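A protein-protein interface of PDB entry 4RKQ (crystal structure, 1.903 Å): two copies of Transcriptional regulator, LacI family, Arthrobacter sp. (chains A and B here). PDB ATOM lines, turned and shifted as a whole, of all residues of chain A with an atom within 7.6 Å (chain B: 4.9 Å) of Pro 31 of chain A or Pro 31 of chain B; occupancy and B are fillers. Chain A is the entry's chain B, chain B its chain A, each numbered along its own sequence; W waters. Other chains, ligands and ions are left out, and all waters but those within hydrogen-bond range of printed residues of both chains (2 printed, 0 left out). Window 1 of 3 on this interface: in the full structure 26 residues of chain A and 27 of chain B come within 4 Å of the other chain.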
ATOM      1  N   ILE A  22     -24.299  22.101   7.381  1.00  0.00           N
ATOM      2  CA  ILE A  22     -25.620  21.921   7.955  1.00  0.00           C
ATOM      3  C   ILE A  22     -25.917  23.048   8.944  1.00  0.00           C
ATOM      4  O   ILE A  22     -24.995  23.565   9.591  1.00  0.00           O
ATOM      5  CB  ILE A  22     -25.768  20.554   8.680  1.00  0.00           C
ATOM      6  CG1 ILE A  22     -24.653  20.348   9.709  1.00  0.00           C
ATOM      7  CG2 ILE A  22     -25.809  19.405   7.655  1.00  0.00           C
ATOM      8  CD1 ILE A  22     -24.847  19.105  10.537  1.00  0.00           C
ATOM      9  N   ASP A  24     -27.659  23.209  11.725  1.00  0.00           N
ATOM     10  CA  ASP A  24     -27.577  22.910  13.152  1.00  0.00           C
ATOM     11  C   ASP A  24     -27.387  21.405  13.343  1.00  0.00           C
ATOM     12  O   ASP A  24     -27.475  20.624  12.394  1.00  0.00           O
ATOM     13  CB  ASP A  24     -28.796  23.414  13.908  1.00  0.00           C
ATOM     14  CG  ASP A  24     -30.019  22.690  13.534  1.00  0.00           C
ATOM     15  OD1 ASP A  24     -30.061  21.462  13.811  1.00  0.00           O
ATOM     16  OD2 ASP A  24     -30.910  23.323  12.916  1.00  0.00           O
ATOM     17  N   LEU A  25     -27.067  21.038  14.571  1.00  0.00           N
ATOM     18  CA  LEU A  25     -26.891  19.640  14.973  1.00  0.00           C
ATOM     19  C   LEU A  25     -27.956  19.305  16.011  1.00  0.00           C
ATOM     20  O   LEU A  25     -28.045  18.172  16.466  1.00  0.00           O
ATOM     21  CB  LEU A  25     -25.484  19.457  15.555  1.00  0.00           C
ATOM     22  CG  LEU A  25     -24.340  19.389  14.561  1.00  0.00           C
ATOM     23  CD1 LEU A  25     -23.005  19.402  15.305  1.00  0.00           C
ATOM     24  CD2 LEU A  25     -24.503  18.109  13.758  1.00  0.00           C
ATOM     25  N   THR A  26     -28.803  20.290  16.349  1.00  0.00           N
ATOM     26  CA  THR A  26     -29.825  20.128  17.394  1.00  0.00           C
ATOM     27  C   THR A  26     -31.173  19.625  16.874  1.00  0.00           C
ATOM     28  O   THR A  26     -31.966  19.090  17.642  1.00  0.00           O
ATOM     29  CB  THR A  26     -30.057  21.463  18.143  1.00  0.00           C
ATOM     30  OG1 THR A  26     -30.336  22.487  17.182  1.00  0.00           O
ATOM     31  CG2 THR A  26     -28.800  21.844  18.960  1.00  0.00           C
ATOM     32  N   ASN A  27     -31.448  19.799  15.588  1.00  0.00           N
ATOM     33  CA  ASN A  27     -32.582  19.119  14.980  1.00  0.00           C
ATOM     34  C   ASN A  27     -32.031  17.766  14.549  1.00  0.00           C
ATOM     35  O   ASN A  27     -31.136  17.747  13.739  1.00  0.00           O
ATOM     36  CB  ASN A  27     -33.075  19.914  13.767  1.00  0.00           C
ATOM     37  CG  ASN A  27     -34.142  19.183  12.935  1.00  0.00           C
ATOM     38  OD1 ASN A  27     -34.445  17.999  13.118  1.00  0.00           O
ATOM     39  ND2 ASN A  27     -34.703  19.914  11.978  1.00  0.00           N
ATOM     40  N   PRO A  28     -32.564  16.644  15.079  1.00  0.00           N
ATOM     41  CA  PRO A  28     -31.920  15.367  14.827  1.00  0.00           C
ATOM     42  C   PRO A  28     -31.932  14.901  13.393  1.00  0.00           C
ATOM     43  O   PRO A  28     -31.201  13.970  13.074  1.00  0.00           O
ATOM     44  CB  PRO A  28     -32.737  14.361  15.668  1.00  0.00           C
ATOM     45  CG  PRO A  28     -33.377  15.186  16.722  1.00  0.00           C
ATOM     46  CD  PRO A  28     -33.643  16.517  16.093  1.00  0.00           C
ATOM     47  N   TYR A  29     -32.755  15.514  12.532  1.00  0.00           N
ATOM     48  CA  TYR A  29     -32.613  15.265  11.109  1.00  0.00           C
ATOM     49  C   TYR A  29     -31.184  15.482  10.619  1.00  0.00           C
ATOM     50  O   TYR A  29     -30.667  14.680   9.850  1.00  0.00           O
ATOM     51  CB  TYR A  29     -33.557  16.123  10.255  1.00  0.00           C
ATOM     52  CG  TYR A  29     -33.284  15.916   8.790  1.00  0.00           C
ATOM     53  CD1 TYR A  29     -33.706  14.762   8.145  1.00  0.00           C
ATOM     54  CD2 TYR A  29     -32.572  16.855   8.043  1.00  0.00           C
ATOM     55  CE1 TYR A  29     -33.445  14.556   6.789  1.00  0.00           C
ATOM     56  CE2 TYR A  29     -32.297  16.643   6.697  1.00  0.00           C
ATOM     57  CZ  TYR A  29     -32.746  15.499   6.076  1.00  0.00           C
ATOM     58  OH  TYR A  29     -32.483  15.279   4.744  1.00  0.00           O
ATOM     59  N   PHE A  30     -30.534  16.570  11.034  1.00  0.00           N
ATOM     60  CA  PHE A  30     -29.250  16.920  10.435  1.00  0.00           C
ATOM     61  C   PHE A  30     -28.075  15.985  10.756  1.00  0.00           C
ATOM     62  O   PHE A  30     -27.328  15.582   9.839  1.00  0.00           O
ATOM     63  CB  PHE A  30     -28.920  18.425  10.653  1.00  0.00           C
ATOM     64  CG  PHE A  30     -29.783  19.295   9.863  1.00  0.00           C
ATOM     65  CD1 PHE A  30     -29.728  19.252   8.466  1.00  0.00           C
ATOM     66  CD2 PHE A  30     -30.714  20.116  10.480  1.00  0.00           C
ATOM     67  CE1 PHE A  30     -30.609  19.985   7.709  1.00  0.00           C
ATOM     68  CE2 PHE A  30     -31.579  20.884   9.714  1.00  0.00           C
ATOM     69  CZ  PHE A  30     -31.517  20.830   8.331  1.00  0.00           C
ATOM     70  N   PRO A  31     -27.944  15.573  12.027  1.00  0.00           N
ATOM     71  CA  PRO A  31     -26.979  14.518  12.269  1.00  0.00           C
ATOM     72  C   PRO A  31     -27.298  13.169  11.586  1.00  0.00           C
ATOM     73  O   PRO A  31     -26.371  12.490  11.209  1.00  0.00           O
ATOM     74  CB  PRO A  31     -26.944  14.375  13.797  1.00  0.00           C
ATOM     75  CG  PRO A  31     -28.012  15.199  14.330  1.00  0.00           C
ATOM     76  CD  PRO A  31     -28.491  16.137  13.281  1.00  0.00           C
ATOM     77  N   ALA A  32     -28.573  12.785  11.412  1.00  0.00           N
ATOM     78  CA  ALA A  32     -28.877  11.597  10.640  1.00  0.00           C
ATOM     79  C   ALA A  32     -28.498  11.749   9.168  1.00  0.00           C
ATOM     80  O   ALA A  32     -27.921  10.854   8.554  1.00  0.00           O
ATOM     81  CB  ALA A  32     -30.356  11.241  10.765  1.00  0.00           C
ATOM     82  N   PHE A  33     -28.773  12.911   8.591  1.00  0.00           N
ATOM     83  CA  PHE A  33     -28.406  13.203   7.216  1.00  0.00           C
ATOM     84  C   PHE A  33     -26.903  13.186   7.068  1.00  0.00           C
ATOM     85  O   PHE A  33     -26.329  12.546   6.163  1.00  0.00           O
ATOM     86  CB  PHE A  33     -28.991  14.553   6.788  1.00  0.00           C
ATOM     87  CG  PHE A  33     -28.383  15.101   5.565  1.00  0.00           C
ATOM     88  CD1 PHE A  33     -28.680  14.580   4.310  1.00  0.00           C
ATOM     89  CD2 PHE A  33     -27.504  16.129   5.654  1.00  0.00           C
ATOM     90  CE1 PHE A  33     -28.096  15.106   3.177  1.00  0.00           C
ATOM     91  CE2 PHE A  33     -26.877  16.614   4.534  1.00  0.00           C
ATOM     92  CZ  PHE A  33     -27.163  16.129   3.305  1.00  0.00           C
ATOM     93  N   ALA A  34     -26.236  13.869   7.975  1.00  0.00           N
ATOM     94  CA  ALA A  34     -24.794  13.915   7.896  1.00  0.00           C
ATOM     95  C   ALA A  34     -24.107  12.536   8.036  1.00  0.00           C
ATOM     96  O   ALA A  34     -23.176  12.232   7.307  1.00  0.00           O
ATOM     97  CB  ALA A  34     -24.232  14.901   8.905  1.00  0.00           C
ATOM     98  N   SER A  35     -24.580  11.746   8.973  1.00  0.00           N
ATOM     99  CA  SER A  35     -24.065  10.422   9.173  1.00  0.00           C
ATOM    100  C   SER A  35     -24.199   9.571   7.909  1.00  0.00           C
ATOM    101  O   SER A  35     -23.279   8.812   7.562  1.00  0.00           O
ATOM    102  CB  SER A  35     -24.750   9.772  10.363  1.00  0.00           C
ATOM    103  OG  SER A  35     -24.312   8.453  10.582  1.00  0.00           O
ATOM    104  N   SER A  36     -25.331   9.668   7.223  1.00  0.00           N
ATOM    105  CA  SER A  36     -25.514   8.964   5.946  1.00  0.00           C
ATOM    106  C   SER A  36     -24.509   9.378   4.871  1.00  0.00           C
ATOM    107  O   SER A  36     -23.894   8.541   4.218  1.00  0.00           O
ATOM    108  CB  SER A  36     -26.934   9.207   5.434  1.00  0.00           C
ATOM    109  OG  SER A  36     -27.094   8.463   4.236  1.00  0.00           O
ATOM    110  N   VAL A  37     -24.312  10.683   4.695  1.00  0.00           N
ATOM    111  CA  VAL A  37     -23.358  11.164   3.711  1.00  0.00           C
ATOM    112  C   VAL A  37     -21.949  10.761   4.064  1.00  0.00           C
ATOM    113  O   VAL A  37     -21.173  10.300   3.204  1.00  0.00           O
ATOM    114  CB  VAL A  37     -23.447  12.676   3.574  1.00  0.00           C
ATOM    115  CG1 VAL A  37     -22.303  13.225   2.746  1.00  0.00           C
ATOM    116  CG2 VAL A  37     -24.808  13.077   3.032  1.00  0.00           C
ATOM    117  N   VAL A  38     -21.618  10.884   5.339  1.00  0.00           N
ATOM    118  CA  VAL A  38     -20.290  10.551   5.770  1.00  0.00           C
ATOM    119  C   VAL A  38     -20.024   9.074   5.517  1.00  0.00           C
ATOM    120  O   VAL A  38     -18.911   8.741   5.148  1.00  0.00           O
ATOM    121  CB  VAL A  38     -20.049  10.918   7.220  1.00  0.00           C
ATOM    122  CG1 VAL A  38     -18.679  10.479   7.678  1.00  0.00           C
ATOM    123  CG2 VAL A  38     -20.164  12.438   7.406  1.00  0.00           C
ATOM    124  N   ASP A  52     -21.119  22.859  11.223  1.00  0.00           N
ATOM    125  CA  ASP A  52     -22.404  23.176  11.793  1.00  0.00           C
ATOM    126  C   ASP A  52     -22.388  24.704  11.962  1.00  0.00           C
ATOM    127  O   ASP A  52     -21.676  25.247  12.802  1.00  0.00           O
ATOM    128  CB  ASP A  52     -22.579  22.490  13.125  1.00  0.00           C
ATOM    129  CG  ASP A  52     -23.666  23.127  14.012  1.00  0.00           C
ATOM    130  OD1 ASP A  52     -24.470  23.952  13.539  1.00  0.00           O
ATOM    131  OD2 ASP A  52     -23.685  22.816  15.218  1.00  0.00           O
ATOM    132  N   HIS A  55     -24.565  28.947  14.607  1.00  0.00           N
ATOM    133  CA  HIS A  55     -24.051  29.619  15.779  1.00  0.00           C
ATOM    134  C   HIS A  55     -23.486  30.973  15.381  1.00  0.00           C
ATOM    135  O   HIS A  55     -23.054  31.155  14.258  1.00  0.00           O
ATOM    136  CB  HIS A  55     -22.926  28.785  16.371  1.00  0.00           C
ATOM    137  CG  HIS A  55     -23.297  27.362  16.642  1.00  0.00           C
ATOM    138  ND1 HIS A  55     -23.917  26.976  17.800  1.00  0.00           N
ATOM    139  CD2 HIS A  55     -23.185  26.241  15.884  1.00  0.00           C
ATOM    140  CE1 HIS A  55     -24.126  25.676  17.783  1.00  0.00           C
ATOM    141  NE2 HIS A  55     -23.720  25.212  16.617  1.00  0.00           N
ATOM    142  N   ILE A 229     -36.979  10.729  11.321  1.00  0.00           N
ATOM    143  CA  ILE A 229     -35.856  10.567  12.278  1.00  0.00           C
ATOM    144  C   ILE A 229     -36.056   9.350  13.208  1.00  0.00           C
ATOM    145  O   ILE A 229     -37.178   9.022  13.589  1.00  0.00           O
ATOM    146  CB  ILE A 229     -35.552  11.860  13.101  1.00  0.00           C
ATOM    147  CG1 ILE A 229     -36.734  12.258  13.986  1.00  0.00           C
ATOM    148  CG2 ILE A 229     -35.159  12.993  12.156  1.00  0.00           C
ATOM    149  CD1 ILE A 229     -36.609  13.581  14.699  1.00  0.00           C
ATOM    150  N   LEU A 246     -33.011   7.865   4.565  1.00  0.00           N
ATOM    151  CA  LEU A 246     -31.765   8.626   4.735  1.00  0.00           C
ATOM    152  C   LEU A 246     -30.612   7.996   3.982  1.00  0.00           C
ATOM    153  O   LEU A 246     -29.721   8.691   3.524  1.00  0.00           O
ATOM    154  CB  LEU A 246     -31.458   8.754   6.236  1.00  0.00           C
ATOM    155  CG  LEU A 246     -32.474   9.690   6.907  1.00  0.00           C
ATOM    156  CD1 LEU A 246     -32.679   9.371   8.379  1.00  0.00           C
ATOM    157  CD2 LEU A 246     -32.004  11.111   6.715  1.00  0.00           C
ATOM    158  N   ASP B  24     -19.530   8.931  16.531  1.00  0.00           N
ATOM    159  CA  ASP B  24     -20.723   8.776  15.698  1.00  0.00           C
ATOM    160  C   ASP B  24     -21.583   9.978  15.893  1.00  0.00           C
ATOM    161  O   ASP B  24     -21.317  10.793  16.764  1.00  0.00           O
ATOM    162  CB  ASP B  24     -21.523   7.505  16.057  1.00  0.00           C
ATOM    163  CG  ASP B  24     -22.031   7.502  17.493  1.00  0.00           C
ATOM    164  OD1 ASP B  24     -22.888   8.345  17.868  1.00  0.00           O
ATOM    165  OD2 ASP B  24     -21.551   6.653  18.262  1.00  0.00           O
ATOM    166  N   LEU B  25     -22.597  10.097  15.044  1.00  0.00           N
ATOM    167  CA  LEU B  25     -23.635  11.132  15.146  1.00  0.00           C
ATOM    168  C   LEU B  25     -25.022  10.504  15.368  1.00  0.00           C
ATOM    169  O   LEU B  25     -26.030  11.172  15.346  1.00  0.00           O
ATOM    170  CB  LEU B  25     -23.660  11.943  13.862  1.00  0.00           C
ATOM    171  CG  LEU B  25     -22.520  12.965  13.662  1.00  0.00           C
ATOM    172  CD1 LEU B  25     -22.434  13.413  12.218  1.00  0.00           C
ATOM    173  CD2 LEU B  25     -22.740  14.143  14.575  1.00  0.00           C
ATOM    174  N   ASN B  27     -25.717   8.423  18.231  1.00  0.00           N
ATOM    175  CA  ASN B  27     -26.040   8.524  19.646  1.00  0.00           C
ATOM    176  C   ASN B  27     -26.253   9.999  19.899  1.00  0.00           C
ATOM    177  O   ASN B  27     -25.327  10.772  19.700  1.00  0.00           O
ATOM    178  CB  ASN B  27     -24.892   7.996  20.467  1.00  0.00           C
ATOM    179  CG  ASN B  27     -25.078   8.238  21.957  1.00  0.00           C
ATOM    180  OD1 ASN B  27     -25.978   8.964  22.393  1.00  0.00           O
ATOM    181  ND2 ASN B  27     -24.182   7.676  22.739  1.00  0.00           N
ATOM    182  N   PRO B  28     -27.483  10.410  20.249  1.00  0.00           N
ATOM    183  CA  PRO B  28     -27.775  11.848  20.335  1.00  0.00           C
ATOM    184  C   PRO B  28     -26.878  12.653  21.284  1.00  0.00           C
ATOM    185  O   PRO B  28     -26.817  13.890  21.161  1.00  0.00           O
ATOM    186  CB  PRO B  28     -29.224  11.889  20.804  1.00  0.00           C
ATOM    187  CG  PRO B  28     -29.796  10.619  20.291  1.00  0.00           C
ATOM    188  CD  PRO B  28     -28.695   9.604  20.437  1.00  0.00           C
ATOM    189  N   TYR B  29     -26.185  11.990  22.214  1.00  0.00           N
ATOM    190  CA  TYR B  29     -25.199  12.689  23.018  1.00  0.00           C
ATOM    191  C   TYR B  29     -24.190  13.417  22.145  1.00  0.00           C
ATOM    192  O   TYR B  29     -23.834  14.537  22.437  1.00  0.00           O
ATOM    193  CB  TYR B  29     -24.458  11.714  23.943  1.00  0.00           C
ATOM    194  CG  TYR B  29     -23.377  12.436  24.693  1.00  0.00           C
ATOM    195  CD1 TYR B  29     -23.702  13.305  25.718  1.00  0.00           C
ATOM    196  CD2 TYR B  29     -22.038  12.322  24.335  1.00  0.00           C
ATOM    197  CE1 TYR B  29     -22.720  14.025  26.370  1.00  0.00           C
ATOM    198  CE2 TYR B  29     -21.040  13.028  25.007  1.00  0.00           C
ATOM    199  CZ  TYR B  29     -21.399  13.906  26.005  1.00  0.00           C
ATOM    200  OH  TYR B  29     -20.439  14.634  26.682  1.00  0.00           O
ATOM    201  N   PHE B  30     -23.699  12.784  21.080  1.00  0.00           N
ATOM    202  CA  PHE B  30     -22.559  13.349  20.369  1.00  0.00           C
ATOM    203  C   PHE B  30     -22.895  14.604  19.580  1.00  0.00           C
ATOM    204  O   PHE B  30     -22.145  15.571  19.665  1.00  0.00           O
ATOM    205  CB  PHE B  30     -21.767  12.295  19.576  1.00  0.00           C
ATOM    206  CG  PHE B  30     -21.033  11.323  20.468  1.00  0.00           C
ATOM    207  CD1 PHE B  30     -20.037  11.761  21.297  1.00  0.00           C
ATOM    208  CD2 PHE B  30     -21.437   9.999  20.567  1.00  0.00           C
ATOM    209  CE1 PHE B  30     -19.408  10.902  22.156  1.00  0.00           C
ATOM    210  CE2 PHE B  30     -20.787   9.122  21.396  1.00  0.00           C
ATOM    211  CZ  PHE B  30     -19.761   9.573  22.197  1.00  0.00           C
ATOM    212  N   PRO B  31     -24.033  14.651  18.915  1.00  0.00           N
ATOM    213  CA  PRO B  31     -24.403  15.932  18.299  1.00  0.00           C
ATOM    214  C   PRO B  31     -24.679  17.031  19.312  1.00  0.00           C
ATOM    215  O   PRO B  31     -24.372  18.165  19.041  1.00  0.00           O
ATOM    216  CB  PRO B  31     -25.666  15.623  17.495  1.00  0.00           C
ATOM    217  CG  PRO B  31     -25.811  14.149  17.504  1.00  0.00           C
ATOM    218  CD  PRO B  31     -24.846  13.519  18.415  1.00  0.00           C
ATOM    219  N   ALA B  32     -25.203  16.674  20.481  1.00  0.00           N
ATOM    220  CA  ALA B  32     -25.448  17.676  21.532  1.00  0.00           C
ATOM    221  C   ALA B  32     -24.148  18.236  22.076  1.00  0.00           C
ATOM    222  O   ALA B  32     -23.978  19.452  22.222  1.00  0.00           O
ATOM    223  CB  ALA B  32     -26.272  17.085  22.635  1.00  0.00           C
ATOM    224  N   PHE B  33     -23.197  17.355  22.325  1.00  0.00           N
ATOM    225  CA  PHE B  33     -21.858  17.749  22.727  1.00  0.00           C
ATOM    226  C   PHE B  33     -21.182  18.609  21.667  1.00  0.00           C
ATOM    227  O   PHE B  33     -20.662  19.682  21.951  1.00  0.00           O
ATOM    228  CB  PHE B  33     -21.005  16.508  23.002  1.00  0.00           C
ATOM    229  CG  PHE B  33     -19.557  16.808  23.177  1.00  0.00           C
ATOM    230  CD1 PHE B  33     -19.103  17.383  24.340  1.00  0.00           C
ATOM    231  CD2 PHE B  33     -18.660  16.504  22.189  1.00  0.00           C
ATOM    232  CE1 PHE B  33     -17.789  17.672  24.524  1.00  0.00           C
ATOM    233  CE2 PHE B  33     -17.338  16.794  22.365  1.00  0.00           C
ATOM    234  CZ  PHE B  33     -16.901  17.370  23.524  1.00  0.00           C
ATOM    235  N   ALA B  34     -21.169  18.136  20.431  1.00  0.00           N
ATOM    236  CA  ALA B  34     -20.570  18.886  19.354  1.00  0.00           C
ATOM    237  C   ALA B  34     -21.175  20.263  19.199  1.00  0.00           C
ATOM    238  O   ALA B  34     -20.424  21.222  19.058  1.00  0.00           O
ATOM    239  CB  ALA B  34     -20.636  18.128  18.028  1.00  0.00           C
ATOM    240  N   SER B  35     -22.497  20.362  19.221  1.00  0.00           N
ATOM    241  CA  SER B  35     -23.167  21.641  19.052  1.00  0.00           C
ATOM    242  C   SER B  35     -22.710  22.617  20.166  1.00  0.00           C
ATOM    243  O   SER B  35     -22.488  23.798  19.928  1.00  0.00           O
ATOM    244  CB  SER B  35     -24.687  21.458  19.137  1.00  0.00           C
ATOM    245  OG  SER B  35     -25.342  22.705  19.019  1.00  0.00           O
HETATM  246  O   HOH W   1     -22.551   8.651  12.612  1.00  0.00           O
HETATM  247  O   HOH W   2     -26.085  23.076  16.376  1.00  0.00           O
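Of the 20 printed residues of chain A, 4 touch a printed residue of chain B.
Hydrophobic or aromatic side chains of chain A within 4 Å of the printed part of chain B: Leu 25, Pro 31 and His 55.
Of the 11 printed residues of chain B, 4 touch a printed residue of chain A.
Hydrophobic or aromatic side chains of chain B within 4 Å of the printed part of chain A: Leu 25, Pro 31 and Ala 34.
Among the printed residues, 6 pairs touch across the chains.
Pro 31 of chain B touches Leu 25 of chain A.
Leu 25 of chain A touches Ala 34 of chain B (CD1 to CB, 3.8 Å).
Ser 35 of chain B touches Thr 26 of chain A (OG to CG2, 3.6 Å).
Leu 25 of chain B touches Pro 31 of chain A (O to CB, 3.7 Å).
Pro 31 of chain A touches Pro 31 of chain B.
O of Ser 35 of chain B touches CE1 of His 55 of chain A, at 3.3 Å.
Water W2 lies within hydrogen-bond range of the side-chain carboxylate of Asp 52 of chain A (2.7 Å), the side-chain hydroxyl of Ser 35 of chain B (2.8 Å), the backbone NH of Leu 25 of chain A (2.9 Å) and a ring nitrogen (NE2) of His 55 of chain A (3.2 Å).
Water W1 bridges OG of Ser 35 of chain A (2.7 Å) and N of Leu 25 of chain B (2.8 Å).
Printed residues of chain B within 4 Å of Leu 25 of chain A: Pro 31 (3.6 Å) and Ala 34 (3.8 Å).
Of the printed residues of chain B, Thr 26 of chain A touches Ser 35 (3.6 Å).
Pro 31 of chain A touches two residues of chain B.
Val 38 of chain A touches none of the printed residues of chain B.
Of the printed residues of chain A, Leu 25 of chain B touches Pro 31 (3.7 Å).
Pro 31 of chain B touches just these residues of chain A: Leu 25 (3.6 Å) and Pro 31 (3.9 Å).
Of the printed residues of chain A, Ala 34 of chain B touches Leu 25 (3.8 Å).
Leu 25 of chain A touches Pro 31 of chain B, and with the chains exchanged Pro 31 of chain A touches Leu 25 of chain B.
Leu 25 of chain A touches Ala 34 of chain B, but with the chains exchanged Ala 34 of chain A does not touch Leu 25 of chain B (4.1 Å).
Pro 31 of chain A touches its own counterpart, Pro 31 of chain B.
11 positions are printed for both chains.
Of the 6 pairs that touch across the chains among the printed residues, 3 have their exchanged pair printed and touching as well.
OD1 of Asp 24 of chain A is in hydrogen-bond range of N of Thr 26 of chain A (3.1 Å).
The side-chain carboxylate of Asp 52 of chain A lies within hydrogen-bond range of a ring nitrogen (NE2) of His 55 of chain A, 2.8 Å away.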
